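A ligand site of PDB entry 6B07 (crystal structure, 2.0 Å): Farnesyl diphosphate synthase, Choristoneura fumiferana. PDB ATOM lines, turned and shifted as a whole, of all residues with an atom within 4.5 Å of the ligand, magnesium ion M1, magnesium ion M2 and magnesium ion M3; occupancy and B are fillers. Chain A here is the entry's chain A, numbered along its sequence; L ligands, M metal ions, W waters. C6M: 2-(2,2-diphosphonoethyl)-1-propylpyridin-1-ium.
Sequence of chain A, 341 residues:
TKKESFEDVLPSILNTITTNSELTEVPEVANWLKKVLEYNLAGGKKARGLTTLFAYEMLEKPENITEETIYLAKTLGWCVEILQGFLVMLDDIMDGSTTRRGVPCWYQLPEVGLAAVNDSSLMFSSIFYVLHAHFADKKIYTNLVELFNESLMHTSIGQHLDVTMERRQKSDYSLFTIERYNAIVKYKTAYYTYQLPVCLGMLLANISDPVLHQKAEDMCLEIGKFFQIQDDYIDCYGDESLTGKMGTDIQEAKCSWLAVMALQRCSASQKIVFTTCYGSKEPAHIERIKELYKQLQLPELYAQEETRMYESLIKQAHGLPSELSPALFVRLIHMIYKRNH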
ATOM      1  N   ARG A  48     -19.376  -4.837  -6.357  1.00  0.00           N
ATOM      2  CA  ARG A  48     -18.884  -4.073  -5.216  1.00  0.00           C
ATOM      3  C   ARG A  48     -18.256  -2.706  -5.642  1.00  0.00           C
ATOM      4  O   ARG A  48     -18.461  -1.714  -4.964  1.00  0.00           O
ATOM      5  CB  ARG A  48     -17.881  -4.897  -4.381  1.00  0.00           C
ATOM      6  CG  ARG A  48     -18.586  -6.070  -3.656  1.00  0.00           C
ATOM      7  CD  ARG A  48     -17.554  -7.054  -3.206  1.00  0.00           C
ATOM      8  NE  ARG A  48     -18.055  -8.343  -2.713  1.00  0.00           N
ATOM      9  CZ  ARG A  48     -18.442  -9.383  -3.467  1.00  0.00           C
ATOM     10  NH1 ARG A  48     -18.486  -9.277  -4.787  1.00  0.00           N
ATOM     11  NH2 ARG A  48     -18.861 -10.531  -2.891  1.00  0.00           N
ATOM     12  N   VAL A  88     -11.078 -13.999  -2.793  1.00  0.00           N
ATOM     13  CA  VAL A  88     -11.507 -15.181  -3.513  1.00  0.00           C
ATOM     14  C   VAL A  88     -10.384 -16.034  -4.056  1.00  0.00           C
ATOM     15  O   VAL A  88     -10.547 -17.249  -4.208  1.00  0.00           O
ATOM     16  CB  VAL A  88     -12.601 -14.971  -4.592  1.00  0.00           C
ATOM     17  CG1 VAL A  88     -13.820 -14.322  -3.987  1.00  0.00           C
ATOM     18  CG2 VAL A  88     -12.084 -14.259  -5.827  1.00  0.00           C
ATOM     19  N   ASP A  91      -9.871 -18.028  -0.932  1.00  0.00           N
ATOM     20  CA  ASP A  91     -11.105 -18.772  -0.701  1.00  0.00           C
ATOM     21  C   ASP A  91     -11.148 -19.991  -1.617  1.00  0.00           C
ATOM     22  O   ASP A  91     -11.459 -21.101  -1.154  1.00  0.00           O
ATOM     23  CB  ASP A  91     -12.303 -17.901  -0.957  1.00  0.00           C
ATOM     24  CG  ASP A  91     -13.619 -18.643  -0.767  1.00  0.00           C
ATOM     25  OD1 ASP A  91     -14.004 -18.844   0.369  1.00  0.00           O
ATOM     26  OD2 ASP A  91     -14.214 -18.999  -1.751  1.00  0.00           O
ATOM     27  N   ASP A  95     -11.545 -23.745  -0.288  1.00  0.00           N
ATOM     28  CA  ASP A  95     -12.819 -24.337  -0.634  1.00  0.00           C
ATOM     29  C   ASP A  95     -12.666 -25.427  -1.676  1.00  0.00           C
ATOM     30  O   ASP A  95     -13.670 -26.074  -2.004  1.00  0.00           O
ATOM     31  CB  ASP A  95     -13.866 -23.279  -1.048  1.00  0.00           C
ATOM     32  CG  ASP A  95     -14.276 -22.418   0.043  1.00  0.00           C
ATOM     33  OD1 ASP A  95     -13.865 -22.672   1.234  1.00  0.00           O
ATOM     34  OD2 ASP A  95     -15.044 -21.397  -0.191  1.00  0.00           O
ATOM     35  N   SER A  97     -11.972 -25.279  -4.726  1.00  0.00           N
ATOM     36  CA  SER A  97     -12.674 -24.907  -5.952  1.00  0.00           C
ATOM     37  C   SER A  97     -11.748 -25.113  -7.155  1.00  0.00           C
ATOM     38  O   SER A  97     -10.566 -25.256  -7.001  1.00  0.00           O
ATOM     39  CB  SER A  97     -13.229 -23.501  -5.836  1.00  0.00           C
ATOM     40  OG  SER A  97     -14.181 -23.312  -4.770  1.00  0.00           O
ATOM     41  N   ARG A 100     -13.605 -20.440 -11.502  1.00  0.00           N
ATOM     42  CA  ARG A 100     -14.245 -19.204 -11.183  1.00  0.00           C
ATOM     43  C   ARG A 100     -14.241 -18.287 -12.471  1.00  0.00           C
ATOM     44  O   ARG A 100     -13.310 -18.397 -13.313  1.00  0.00           O
ATOM     45  CB  ARG A 100     -13.551 -18.485 -10.050  1.00  0.00           C
ATOM     46  CG  ARG A 100     -14.355 -17.234  -9.707  1.00  0.00           C
ATOM     47  CD  ARG A 100     -13.864 -16.517  -8.522  1.00  0.00           C
ATOM     48  NE  ARG A 100     -13.922 -17.355  -7.358  1.00  0.00           N
ATOM     49  CZ  ARG A 100     -14.911 -17.334  -6.453  1.00  0.00           C
ATOM     50  NH1 ARG A 100     -15.971 -16.560  -6.593  1.00  0.00           N
ATOM     51  NH2 ARG A 100     -14.826 -18.086  -5.380  1.00  0.00           N
ATOM     52  N   THR A 155     -13.595  -9.982   7.496  1.00  0.00           N
ATOM     53  CA  THR A 155     -13.675 -11.077   6.562  1.00  0.00           C
ATOM     54  C   THR A 155     -12.961 -12.343   7.025  1.00  0.00           C
ATOM     55  O   THR A 155     -13.471 -13.438   6.852  1.00  0.00           O
ATOM     56  CB  THR A 155     -13.249 -10.666   5.144  1.00  0.00           C
ATOM     57  OG1 THR A 155     -13.923  -9.461   4.736  1.00  0.00           O
ATOM     58  CG2 THR A 155     -13.559 -11.697   4.193  1.00  0.00           C
ATOM     59  N   GLN A 159     -14.296 -15.982   7.692  1.00  0.00           N
ATOM     60  CA  GLN A 159     -13.705 -17.137   7.034  1.00  0.00           C
ATOM     61  C   GLN A 159     -13.239 -18.183   8.039  1.00  0.00           C
ATOM     62  O   GLN A 159     -13.312 -19.385   7.764  1.00  0.00           O
ATOM     63  CB  GLN A 159     -12.494 -16.789   6.145  1.00  0.00           C
ATOM     64  CG  GLN A 159     -12.852 -16.006   4.896  1.00  0.00           C
ATOM     65  CD  GLN A 159     -13.665 -16.793   3.869  1.00  0.00           C
ATOM     66  OE1 GLN A 159     -14.851 -17.063   4.082  1.00  0.00           O
ATOM     67  NE2 GLN A 159     -13.048 -17.173   2.795  1.00  0.00           N
ATOM     68  N   ASP A 162     -16.345 -20.126   8.913  1.00  0.00           N
ATOM     69  CA  ASP A 162     -16.705 -20.883   7.737  1.00  0.00           C
ATOM     70  C   ASP A 162     -15.942 -22.146   7.540  1.00  0.00           C
ATOM     71  O   ASP A 162     -16.564 -23.183   7.251  1.00  0.00           O
ATOM     72  CB  ASP A 162     -16.543 -19.967   6.497  1.00  0.00           C
ATOM     73  CG  ASP A 162     -16.895 -20.640   5.190  1.00  0.00           C
ATOM     74  OD1 ASP A 162     -16.071 -21.433   4.674  1.00  0.00           O
ATOM     75  OD2 ASP A 162     -17.992 -20.348   4.634  1.00  0.00           O
ATOM     76  N   LYS A 188     -18.039 -12.770   7.100  1.00  0.00           N
ATOM     77  CA  LYS A 188     -17.312 -13.134   5.924  1.00  0.00           C
ATOM     78  C   LYS A 188     -17.808 -12.366   4.688  1.00  0.00           C
ATOM     79  O   LYS A 188     -17.075 -12.268   3.726  1.00  0.00           O
ATOM     80  CB  LYS A 188     -17.363 -14.648   5.625  1.00  0.00           C
ATOM     81  CG  LYS A 188     -18.544 -15.159   4.838  1.00  0.00           C
ATOM     82  CD  LYS A 188     -18.414 -16.595   4.383  1.00  0.00           C
ATOM     83  CE  LYS A 188     -19.747 -17.167   3.820  1.00  0.00           C
ATOM     84  NZ  LYS A 188     -19.559 -18.437   3.043  1.00  0.00           N
ATOM     85  N   THR A 189     -19.054 -11.888   4.711  1.00  0.00           N
ATOM     86  CA  THR A 189     -19.678 -11.310   3.449  1.00  0.00           C
ATOM     87  C   THR A 189     -20.208  -9.934   3.642  1.00  0.00           C
ATOM     88  O   THR A 189     -19.866  -9.083   2.870  1.00  0.00           O
ATOM     89  CB  THR A 189     -20.786 -12.202   2.926  1.00  0.00           C
ATOM     90  OG1 THR A 189     -20.217 -13.422   2.507  1.00  0.00           O
ATOM     91  CG2 THR A 189     -21.597 -11.544   1.741  1.00  0.00           C
ATOM     92  N   TYR A 192     -17.617  -6.647   3.903  1.00  0.00           N
ATOM     93  CA  TYR A 192     -16.835  -6.213   2.734  1.00  0.00           C
ATOM     94  C   TYR A 192     -17.689  -5.979   1.499  1.00  0.00           C
ATOM     95  O   TYR A 192     -17.329  -5.126   0.643  1.00  0.00           O
ATOM     96  CB  TYR A 192     -15.634  -7.148   2.426  1.00  0.00           C
ATOM     97  CG  TYR A 192     -15.828  -8.227   1.451  1.00  0.00           C
ATOM     98  CD1 TYR A 192     -16.318  -9.463   1.851  1.00  0.00           C
ATOM     99  CD2 TYR A 192     -15.579  -8.050   0.163  1.00  0.00           C
ATOM    100  CE1 TYR A 192     -16.527 -10.472   0.968  1.00  0.00           C
ATOM    101  CE2 TYR A 192     -15.785  -9.047  -0.772  1.00  0.00           C
ATOM    102  CZ  TYR A 192     -16.258 -10.258  -0.361  1.00  0.00           C
ATOM    103  OH  TYR A 192     -16.448 -11.299  -1.248  1.00  0.00           O
ATOM    104  N   THR A 193     -18.809  -6.705   1.412  1.00  0.00           N
ATOM    105  CA  THR A 193     -19.664  -6.643   0.245  1.00  0.00           C
ATOM    106  C   THR A 193     -20.535  -5.390   0.206  1.00  0.00           C
ATOM    107  O   THR A 193     -20.728  -4.882  -0.904  1.00  0.00           O
ATOM    108  CB  THR A 193     -20.441  -7.950   0.070  1.00  0.00           C
ATOM    109  OG1 THR A 193     -19.466  -8.979  -0.088  1.00  0.00           O
ATOM    110  CG2 THR A 193     -21.223  -7.991  -1.182  1.00  0.00           C
ATOM    111  N   PHE A 227     -27.770 -11.344   0.663  1.00  0.00           N
ATOM    112  CA  PHE A 227     -26.902 -11.647  -0.466  1.00  0.00           C
ATOM    113  C   PHE A 227     -26.177 -13.015  -0.347  1.00  0.00           C
ATOM    114  O   PHE A 227     -26.091 -13.799  -1.313  1.00  0.00           O
ATOM    115  CB  PHE A 227     -25.857 -10.506  -0.634  1.00  0.00           C
ATOM    116  CG  PHE A 227     -25.029 -10.641  -1.889  1.00  0.00           C
ATOM    117  CD1 PHE A 227     -25.530 -10.206  -3.123  1.00  0.00           C
ATOM    118  CD2 PHE A 227     -23.750 -11.225  -1.864  1.00  0.00           C
ATOM    119  CE1 PHE A 227     -24.783 -10.315  -4.278  1.00  0.00           C
ATOM    120  CE2 PHE A 227     -23.017 -11.384  -3.048  1.00  0.00           C
ATOM    121  CZ  PHE A 227     -23.533 -10.889  -4.265  1.00  0.00           C
ATOM    122  N   GLN A 228     -25.701 -13.351   0.859  1.00  0.00           N
ATOM    123  CA  GLN A 228     -25.029 -14.675   1.023  1.00  0.00           C
ATOM    124  C   GLN A 228     -25.993 -15.865   0.996  1.00  0.00           C
ATOM    125  O   GLN A 228     -25.645 -17.008   0.588  1.00  0.00           O
ATOM    126  CB  GLN A 228     -24.239 -14.681   2.329  1.00  0.00           C
ATOM    127  CG  GLN A 228     -23.366 -15.891   2.487  1.00  0.00           C
ATOM    128  CD  GLN A 228     -22.397 -16.009   1.370  1.00  0.00           C
ATOM    129  OE1 GLN A 228     -21.802 -15.015   0.996  1.00  0.00           O
ATOM    130  NE2 GLN A 228     -22.192 -17.195   0.859  1.00  0.00           N
ATOM    131  N   ASP A 231     -26.134 -16.407  -2.512  1.00  0.00           N
ATOM    132  CA  ASP A 231     -24.895 -17.132  -2.926  1.00  0.00           C
ATOM    133  C   ASP A 231     -24.977 -18.662  -2.608  1.00  0.00           C
ATOM    134  O   ASP A 231     -24.646 -19.532  -3.415  1.00  0.00           O
ATOM    135  CB  ASP A 231     -23.680 -16.516  -2.192  1.00  0.00           C
ATOM    136  CG  ASP A 231     -22.394 -17.063  -2.726  1.00  0.00           C
ATOM    137  OD1 ASP A 231     -22.076 -16.693  -3.885  1.00  0.00           O
ATOM    138  OD2 ASP A 231     -21.750 -17.892  -2.004  1.00  0.00           O
ATOM    139  N   ASP A 235     -25.087 -21.865  -5.192  1.00  0.00           N
ATOM    140  CA  ASP A 235     -24.076 -22.915  -5.169  1.00  0.00           C
ATOM    141  C   ASP A 235     -24.693 -24.215  -5.588  1.00  0.00           C
ATOM    142  O   ASP A 235     -24.062 -24.995  -6.304  1.00  0.00           O
ATOM    143  CB  ASP A 235     -23.421 -23.091  -3.787  1.00  0.00           C
ATOM    144  CG  ASP A 235     -22.147 -23.892  -3.859  1.00  0.00           C
ATOM    145  OD1 ASP A 235     -21.186 -23.259  -4.308  1.00  0.00           O
ATOM    146  OD2 ASP A 235     -22.114 -25.138  -3.561  1.00  0.00           O
ATOM    147  N   LYS A 245     -18.774 -21.025 -12.058  1.00  0.00           N
ATOM    148  CA  LYS A 245     -18.098 -21.780 -10.998  1.00  0.00           C
ATOM    149  C   LYS A 245     -18.891 -23.044 -10.644  1.00  0.00           C
ATOM    150  O   LYS A 245     -20.115 -23.060 -10.636  1.00  0.00           O
ATOM    151  CB  LYS A 245     -17.770 -20.905  -9.748  1.00  0.00           C
ATOM    152  CG  LYS A 245     -18.974 -20.301  -9.094  1.00  0.00           C
ATOM    153  CD  LYS A 245     -18.670 -19.354  -7.906  1.00  0.00           C
ATOM    154  CE  LYS A 245     -19.529 -19.608  -6.648  1.00  0.00           C
ATOM    155  NZ  LYS A 245     -20.515 -18.507  -6.334  1.00  0.00           N
ATOM    156  N   ASP A 249     -20.224 -26.447  -1.900  1.00  0.00           N
ATOM    157  CA  ASP A 249     -20.720 -26.383  -0.537  1.00  0.00           C
ATOM    158  C   ASP A 249     -21.061 -27.785   0.062  1.00  0.00           C
ATOM    159  O   ASP A 249     -20.701 -28.077   1.247  1.00  0.00           O
ATOM    160  CB  ASP A 249     -21.927 -25.475  -0.452  1.00  0.00           C
ATOM    161  CG  ASP A 249     -21.549 -23.996  -0.545  1.00  0.00           C
ATOM    162  OD1 ASP A 249     -20.318 -23.699  -0.523  1.00  0.00           O
ATOM    163  OD2 ASP A 249     -22.490 -23.150  -0.553  1.00  0.00           O
ATOM    164  N   LYS A 254     -20.251 -27.486   4.072  1.00  0.00           N
ATOM    165  CA  LYS A 254     -20.419 -26.124   4.540  1.00  0.00           C
ATOM    166  C   LYS A 254     -21.737 -25.941   5.307  1.00  0.00           C
ATOM    167  O   LYS A 254     -22.743 -26.584   5.009  1.00  0.00           O
ATOM    168  CB  LYS A 254     -20.369 -25.098   3.363  1.00  0.00           C
ATOM    169  CG  LYS A 254     -19.045 -25.046   2.566  1.00  0.00           C
ATOM    170  CD  LYS A 254     -17.841 -24.556   3.401  1.00  0.00           C
ATOM    171  CE  LYS A 254     -16.626 -24.334   2.464  1.00  0.00           C
ATOM    172  NZ  LYS A 254     -15.547 -23.734   3.229  1.00  0.00           N
HETATM  173  OAN C6M L   1     -16.851 -19.477  -0.551  1.00  0.00           O
HETATM  174  PAL C6M L   1     -18.099 -18.551  -0.430  1.00  0.00           P
HETATM  175  OAO C6M L   1     -19.305 -19.475  -0.784  1.00  0.00           O
HETATM  176  OAM C6M L   1     -18.361 -17.743   0.801  1.00  0.00           O
HETATM  177  CAK C6M L   1     -18.096 -17.406  -1.876  1.00  0.00           C
HETATM  178  PAP C6M L   1     -18.013 -18.326  -3.432  1.00  0.00           P
HETATM  179  OAR C6M L   1     -19.329 -19.158  -3.683  1.00  0.00           O
HETATM  180  OAS C6M L   1     -16.882 -19.406  -3.543  1.00  0.00           O
HETATM  181  OAQ C6M L   1     -17.756 -17.253  -4.496  1.00  0.00           O
HETATM  182  CAJ C6M L   1     -16.920 -16.333  -1.925  1.00  0.00           C
HETATM  183  CAF C6M L   1     -16.632 -15.644  -0.725  1.00  0.00           C
HETATM  184  CAE C6M L   1     -15.360 -15.739  -0.196  1.00  0.00           C
HETATM  185  CAD C6M L   1     -14.981 -15.092   0.955  1.00  0.00           C
HETATM  186  CAC C6M L   1     -15.877 -14.357   1.659  1.00  0.00           C
HETATM  187  CAB C6M L   1     -17.137 -14.210   1.143  1.00  0.00           C
HETATM  188  NAA C6M L   1     -17.491 -14.843  -0.022  1.00  0.00           N
HETATM  189  CAG C6M L   1     -18.859 -14.681  -0.441  1.00  0.00           C
HETATM  190  CAH C6M L   1     -19.136 -13.303  -0.943  1.00  0.00           C
HETATM  191  CAI C6M L   1     -20.536 -13.379  -1.643  1.00  0.00           C
HETATM  192 MG    MG M   1     -15.702 -19.882   1.153  1.00  0.00          MG
HETATM  193 MG    MG M   2     -15.904 -20.314  -2.061  1.00  0.00          MG
HETATM  194 MG    MG M   3     -20.696 -19.627  -2.282  1.00  0.00          MG
HETATM  195  O   HOH W   1     -20.014 -21.698  -2.530  1.00  0.00           O
HETATM  196  O   HOH W   2     -16.229 -18.439   2.377  1.00  0.00           O
HETATM  197  O   HOH W   3     -17.162 -21.918  -2.177  1.00  0.00           O
HETATM  198  O   HOH W   4     -19.598 -21.462   0.972  1.00  0.00           O
HETATM  199  O   HOH W   5     -14.350 -20.590   2.628  1.00  0.00           O
HETATM  200  O   HOH W   6     -21.979 -20.080  -4.079  1.00  0.00           O
HETATM  201  O   HOH W   7     -17.010 -21.189  -5.543  1.00  0.00           O
HETATM  202  O   HOH W   8     -17.119 -21.370   1.941  1.00  0.00           O
HETATM  203  O   HOH W   9     -19.781 -15.475  -4.505  1.00  0.00           O
HETATM  204  O   HOH W  10     -18.589 -12.946  -4.458  1.00  0.00           O
HETATM  205  O   HOH W  11     -14.671 -21.203  -3.462  1.00  0.00           O
HETATM  206  O   HOH W  12     -22.198 -20.532  -0.912  1.00  0.00           O
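NZ of Lys 245 lies within salt-bridge range of OAQ of the ligand, 3.5 Å away.
NH1 of Arg 100 is in salt-bridge range of OAQ of the ligand (2.8 Å).
An oxygen (OAM) of the ligand lies within salt-bridge range of the side-chain amino group (NZ) of Lys 188, 2.6 Å away.
The guanidinium group (NE) of Arg 48 sits at hydrogen-bond distance from the side-chain hydroxyl (OG1) of Thr 193 (3.0 Å).
NZ of Lys 188 lies within salt-bridge range of OD2 of Asp 162 (2.9 Å).
OD2 of Asp 91 sits close to NH2 of Arg 100.
NZ of Lys 245 lies within salt-bridge range of OD1 of Asp 231 (3.4 Å).
The side-chain hydroxyl of Thr 189 lies within hydrogen-bond range of the side-chain amide oxygen of Gln 228 (2.7 Å).
The side-chain amino group (NZ) of Lys 254 lies within salt-bridge range of the side-chain carboxylate (OD1) of Asp 95 (2.8 Å).
NZ of Lys 254 lies within salt-bridge range of OD1 of Asp 162 (2.8 Å).
OH of Tyr 192 sits at hydrogen-bond distance from NH2 of Arg 48 (3.0 Å).
Arg 48 touches the ligand.
Gln 159 touches the ligand.
Thr 189 touches the ligand (OG1 to CAB, 3.5 Å).
Tyr 192 touches the ligand.
Phe 227 touches the ligand.
Gln 228 touches the ligand.
The nearest printed residue that does not touch the ligand is Val 88 (4.2 Å).
OD1 of Asp 162 touches magnesium ion M1 (3.9 Å).
Of the 20 residues printed, 3 come within 4 Å of magnesium ion M1.
The nearest printed residue that does not touch magnesium ion M1 is Gln 159 (4.1 Å).
Of the 20 residues printed, 2 come within 4 Å of magnesium ion M2.
Along chain A the residues within 4 Å of magnesium ion M2 span positions 91 to 95.
The nearest printed residue that does not touch magnesium ion M2 is Arg 100 (4.1 Å).
Within 4 Å of magnesium ion M3: Asp 231.
The nearest printed residue that does not touch magnesium ion M3 is Asp 235 (4.2 Å).
Magnesium ion M1 is bound by water W2 (2.0 Å), an oxygen (OAN) of the ligand (2.1 Å), water W5 (2.1 Å), the side-chain carboxylate of Asp 95 (2.1 Å), the side-chain carboxylate of Asp 91 (2.1 Å) and water W8 (2.2 Å).
Magnesium ion M2 is bound by OAN of the ligand (2.0 Å), OAS of the ligand (2.0 Å), water W3 (2.0 Å), water W11 (2.1 Å), OD2 of Asp 91 (2.2 Å) and OD2 of Asp 95 (2.3 Å).
Magnesium ion M3 is bound by OAR of the ligand (2.0 Å).
The side-chain carboxylate (OD2) of Asp 231 binds magnesium ion M3, 2.0 Å away.
Magnesium ion M3 is bound by an oxygen (OAO) of the ligand (2.0 Å).
Water W1 binds magnesium ion M3, 2.2 Å away.
Water W12 is bound to magnesium ion M3, at 2.2 Å.
Magnesium ion M3 is bound by water W6 (2.3 Å).
Water W8 lies within hydrogen-bond range of the side-chain carboxylate of Asp 162 and the side-chain amino group of Lys 254.
Water W5 lies within hydrogen-bond range of the side-chain carboxylate of Asp 95, the side-chain carboxylate of Asp 162 and the side-chain amino group of Lys 254.
Water W2 lies within hydrogen-bond range of the side-chain amide oxygen (OE1) of Gln 159, an oxygen (OAM) of the ligand, the side-chain amino group (NZ) of Lys 188 and the side-chain carboxylate (OD2) of Asp 162.
Water W1 lies within hydrogen-bond range of the side-chain carboxylate of Asp 235 (2.6 Å) and the side-chain carboxylate of Asp 249 (2.9 Å).
Water W6 lies within hydrogen-bond range of the backbone carbonyl oxygen (O) of Asp 231, the side-chain amino group (NZ) of Lys 245 and the side-chain carboxylate (OD1) of Asp 235.
Water W9 lies within hydrogen-bond range of the side-chain carboxylate of Asp 231 (2.7 Å) and an oxygen (OAQ) of the ligand (2.7 Å).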
